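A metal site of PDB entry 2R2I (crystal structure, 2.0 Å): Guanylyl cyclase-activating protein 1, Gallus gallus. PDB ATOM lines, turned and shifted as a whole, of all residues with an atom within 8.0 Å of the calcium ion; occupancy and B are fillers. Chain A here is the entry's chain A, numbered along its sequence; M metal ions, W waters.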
ATOM      1  N   CYS A 104      -3.652  25.823 -21.135  1.00  0.00           N
ATOM      2  CA  CYS A 104      -5.056  25.961 -21.503  1.00  0.00           C
ATOM      3  C   CYS A 104      -5.947  26.005 -20.274  1.00  0.00           C
ATOM      4  O   CYS A 104      -5.664  25.350 -19.269  1.00  0.00           O
ATOM      5  CB  CYS A 104      -5.472  24.768 -22.374  1.00  0.00           C
ATOM      6  SG  CYS A 104      -4.335  24.407 -23.743  1.00  0.00           S
ATOM      7  N   ILE A 105      -7.033  26.765 -20.345  1.00  0.00           N
ATOM      8  CA  ILE A 105      -7.976  26.834 -19.233  1.00  0.00           C
ATOM      9  C   ILE A 105      -9.188  25.969 -19.575  1.00  0.00           C
ATOM     10  O   ILE A 105      -9.924  26.284 -20.499  1.00  0.00           O
ATOM     11  CB  ILE A 105      -8.513  28.269 -18.994  1.00  0.00           C
ATOM     12  CG1 ILE A 105      -7.367  29.225 -18.674  1.00  0.00           C
ATOM     13  CG2 ILE A 105      -9.534  28.248 -17.847  1.00  0.00           C
ATOM     14  CD1 ILE A 105      -7.798  30.682 -18.571  1.00  0.00           C
ATOM     15  N   PHE A 137     -17.462  29.957 -21.738  1.00  0.00           N
ATOM     16  CA  PHE A 137     -17.117  29.053 -22.829  1.00  0.00           C
ATOM     17  C   PHE A 137     -18.069  29.205 -24.009  1.00  0.00           C
ATOM     18  O   PHE A 137     -17.642  29.211 -25.171  1.00  0.00           O
ATOM     19  CB  PHE A 137     -17.077  27.606 -22.324  1.00  0.00           C
ATOM     20  CG  PHE A 137     -15.777  27.228 -21.671  1.00  0.00           C
ATOM     21  CD1 PHE A 137     -14.776  26.586 -22.401  1.00  0.00           C
ATOM     22  CD2 PHE A 137     -15.515  27.572 -20.344  1.00  0.00           C
ATOM     23  CE1 PHE A 137     -13.545  26.279 -21.821  1.00  0.00           C
ATOM     24  CE2 PHE A 137     -14.279  27.267 -19.755  1.00  0.00           C
ATOM     25  CZ  PHE A 137     -13.294  26.615 -20.498  1.00  0.00           C
ATOM     26  N   ILE A 140     -16.690  32.696 -25.451  1.00  0.00           N
ATOM     27  CA  ILE A 140     -15.321  32.881 -25.942  1.00  0.00           C
ATOM     28  C   ILE A 140     -14.505  31.653 -26.317  1.00  0.00           C
ATOM     29  O   ILE A 140     -13.351  31.785 -26.726  1.00  0.00           O
ATOM     30  CB  ILE A 140     -14.496  33.781 -24.978  1.00  0.00           C
ATOM     31  CG1 ILE A 140     -14.177  33.040 -23.688  1.00  0.00           C
ATOM     32  CG2 ILE A 140     -15.274  35.040 -24.662  1.00  0.00           C
ATOM     33  CD1 ILE A 140     -13.232  33.820 -22.778  1.00  0.00           C
ATOM     34  N   ASP A 141     -15.067  30.458 -26.165  1.00  0.00           N
ATOM     35  CA  ASP A 141     -14.358  29.245 -26.559  1.00  0.00           C
ATOM     36  C   ASP A 141     -14.752  29.057 -28.027  1.00  0.00           C
ATOM     37  O   ASP A 141     -15.552  28.174 -28.372  1.00  0.00           O
ATOM     38  CB  ASP A 141     -14.804  28.047 -25.715  1.00  0.00           C
ATOM     39  CG  ASP A 141     -14.221  26.737 -26.197  1.00  0.00           C
ATOM     40  OD1 ASP A 141     -13.194  26.767 -26.895  1.00  0.00           O
ATOM     41  OD2 ASP A 141     -14.802  25.668 -25.871  1.00  0.00           O
ATOM     42  N   ILE A 142     -14.195  29.921 -28.874  1.00  0.00           N
ATOM     43  CA  ILE A 142     -14.474  29.959 -30.300  1.00  0.00           C
ATOM     44  C   ILE A 142     -14.572  28.626 -31.046  1.00  0.00           C
ATOM     45  O   ILE A 142     -15.533  28.392 -31.763  1.00  0.00           O
ATOM     46  CB  ILE A 142     -13.436  30.861 -31.027  1.00  0.00           C
ATOM     47  CG1 ILE A 142     -13.386  32.231 -30.356  1.00  0.00           C
ATOM     48  CG2 ILE A 142     -13.804  31.025 -32.494  1.00  0.00           C
ATOM     49  CD1 ILE A 142     -14.720  32.934 -30.271  1.00  0.00           C
ATOM     50  N   ASN A 143     -13.583  27.758 -30.882  1.00  0.00           N
ATOM     51  CA  ASN A 143     -13.626  26.481 -31.588  1.00  0.00           C
ATOM     52  C   ASN A 143     -14.320  25.366 -30.800  1.00  0.00           C
ATOM     53  O   ASN A 143     -14.269  24.203 -31.191  1.00  0.00           O
ATOM     54  CB  ASN A 143     -12.204  26.056 -31.981  1.00  0.00           C
ATOM     55  CG  ASN A 143     -11.361  25.664 -30.785  1.00  0.00           C
ATOM     56  OD1 ASN A 143     -11.607  26.090 -29.660  1.00  0.00           O
ATOM     57  ND2 ASN A 143     -10.333  24.850 -31.037  1.00  0.00           N
ATOM     58  N   GLY A 144     -14.970  25.747 -29.706  1.00  0.00           N
ATOM     59  CA  GLY A 144     -15.703  24.806 -28.870  1.00  0.00           C
ATOM     60  C   GLY A 144     -15.059  23.487 -28.472  1.00  0.00           C
ATOM     61  O   GLY A 144     -15.720  22.446 -28.476  1.00  0.00           O
ATOM     62  N   ASP A 145     -13.783  23.518 -28.113  1.00  0.00           N
ATOM     63  CA  ASP A 145     -13.103  22.282 -27.717  1.00  0.00           C
ATOM     64  C   ASP A 145     -13.057  22.048 -26.203  1.00  0.00           C
ATOM     65  O   ASP A 145     -12.497  21.063 -25.736  1.00  0.00           O
ATOM     66  CB  ASP A 145     -11.685  22.257 -28.299  1.00  0.00           C
ATOM     67  CG  ASP A 145     -10.822  23.393 -27.790  1.00  0.00           C
ATOM     68  OD1 ASP A 145     -11.354  24.312 -27.123  1.00  0.00           O
ATOM     69  OD2 ASP A 145      -9.606  23.386 -28.063  1.00  0.00           O
ATOM     70  N   GLY A 146     -13.668  22.953 -25.437  1.00  0.00           N
ATOM     71  CA  GLY A 146     -13.678  22.796 -23.991  1.00  0.00           C
ATOM     72  C   GLY A 146     -12.421  23.335 -23.316  1.00  0.00           C
ATOM     73  O   GLY A 146     -12.174  23.083 -22.133  1.00  0.00           O
ATOM     74  N   GLU A 147     -11.618  24.063 -24.083  1.00  0.00           N
ATOM     75  CA  GLU A 147     -10.398  24.638 -23.533  1.00  0.00           C
ATOM     76  C   GLU A 147     -10.278  26.079 -24.012  1.00  0.00           C
ATOM     77  O   GLU A 147     -10.708  26.408 -25.111  1.00  0.00           O
ATOM     78  CB  GLU A 147      -9.174  23.867 -24.037  1.00  0.00           C
ATOM     79  CG  GLU A 147      -9.190  22.382 -23.769  1.00  0.00           C
ATOM     80  CD  GLU A 147      -8.034  21.683 -24.472  1.00  0.00           C
ATOM     81  OE1 GLU A 147      -8.212  21.209 -25.618  1.00  0.00           O
ATOM     82  OE2 GLU A 147      -6.940  21.643 -23.872  1.00  0.00           O
ATOM     83  N   LEU A 148      -9.697  26.929 -23.179  1.00  0.00           N
ATOM     84  CA  LEU A 148      -9.482  28.327 -23.558  1.00  0.00           C
ATOM     85  C   LEU A 148      -7.984  28.545 -23.768  1.00  0.00           C
ATOM     86  O   LEU A 148      -7.191  28.374 -22.834  1.00  0.00           O
ATOM     87  CB  LEU A 148      -9.968  29.284 -22.478  1.00  0.00           C
ATOM     88  CG  LEU A 148     -11.434  29.259 -22.067  1.00  0.00           C
ATOM     89  CD1 LEU A 148     -11.668  30.350 -21.049  1.00  0.00           C
ATOM     90  CD2 LEU A 148     -12.328  29.452 -23.284  1.00  0.00           C
ATOM     91  N   SER A 149      -7.585  28.921 -24.974  1.00  0.00           N
ATOM     92  CA  SER A 149      -6.183  29.202 -25.242  1.00  0.00           C
ATOM     93  C   SER A 149      -5.963  30.625 -24.723  1.00  0.00           C
ATOM     94  O   SER A 149      -6.926  31.348 -24.448  1.00  0.00           O
ATOM     95  CB  SER A 149      -5.899  29.160 -26.743  1.00  0.00           C
ATOM     96  OG  SER A 149      -6.620  30.180 -27.422  1.00  0.00           O
ATOM     97  N   GLU A 152      -7.778  32.951 -27.097  1.00  0.00           N
ATOM     98  CA  GLU A 152      -9.217  33.049 -26.918  1.00  0.00           C
ATOM     99  C   GLU A 152      -9.550  33.875 -25.680  1.00  0.00           C
ATOM    100  O   GLU A 152     -10.459  34.709 -25.695  1.00  0.00           O
ATOM    101  CB  GLU A 152      -9.835  31.653 -26.797  1.00  0.00           C
ATOM    102  CG  GLU A 152      -9.731  30.825 -28.070  1.00  0.00           C
ATOM    103  CD  GLU A 152     -10.212  29.403 -27.873  1.00  0.00           C
ATOM    104  OE1 GLU A 152      -9.875  28.804 -26.828  1.00  0.00           O
ATOM    105  OE2 GLU A 152     -10.914  28.874 -28.753  1.00  0.00           O
ATOM    106  N   PHE A 153      -8.802  33.637 -24.609  1.00  0.00           N
ATOM    107  CA  PHE A 153      -8.995  34.348 -23.345  1.00  0.00           C
ATOM    108  C   PHE A 153      -8.850  35.851 -23.544  1.00  0.00           C
ATOM    109  O   PHE A 153      -9.792  36.620 -23.358  1.00  0.00           O
ATOM    110  CB  PHE A 153      -7.985  33.865 -22.313  1.00  0.00           C
ATOM    111  CG  PHE A 153      -8.173  34.474 -20.939  1.00  0.00           C
ATOM    112  CD1 PHE A 153      -9.182  34.022 -20.099  1.00  0.00           C
ATOM    113  CD2 PHE A 153      -7.330  35.483 -20.494  1.00  0.00           C
ATOM    114  CE1 PHE A 153      -9.358  34.577 -18.832  1.00  0.00           C
ATOM    115  CE2 PHE A 153      -7.488  36.049 -19.228  1.00  0.00           C
ATOM    116  CZ  PHE A 153      -8.502  35.596 -18.397  1.00  0.00           C
HETATM  117 CA    CA M   1     -10.921  26.631 -27.392  1.00  0.00          CA
HETATM  118  O   HOH W   1      -8.717  25.868 -28.046  1.00  0.00           O
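Within 4 Å of the calcium ion: Asp 141, Asn 143, Asp 145, Glu 147 and Glu 152.
The nearest printed residue that does not touch the calcium ion is Leu 148 (4.4 Å).
The backbone NH (N) of Gly 146 sits at hydrogen-bond distance from the side-chain carboxylate (OD2) of Asp 141, at 3.0 Å.
The side-chain carboxylate (OE2) of Glu 152 sits close to the backbone NH (N) of Ile 142 (3.4 Å).
The backbone NH of Glu 152 lies within hydrogen-bond range of the side-chain hydroxyl of Ser 149 (3.0 Å).
OD1 of Asp 141 lies close to N of Gly 144.
The calcium ion is bound by the backbone carbonyl oxygen (O) of Glu 147 (2.3 Å), the side-chain carboxylate (OD1) of Asp 141 (2.3 Å), the side-chain carboxylate (OD1) of Asp 145 (2.4 Å), water W1 (2.4 Å), the side-chain amide oxygen (OD1) of Asn 143 (2.4 Å), the side-chain carboxylate (OE1) of Glu 152 (2.5 Å) and the side-chain carboxylate (OE2) of Glu 152 (2.6 Å).
The calcium ion has seven donor atoms within binding distance.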
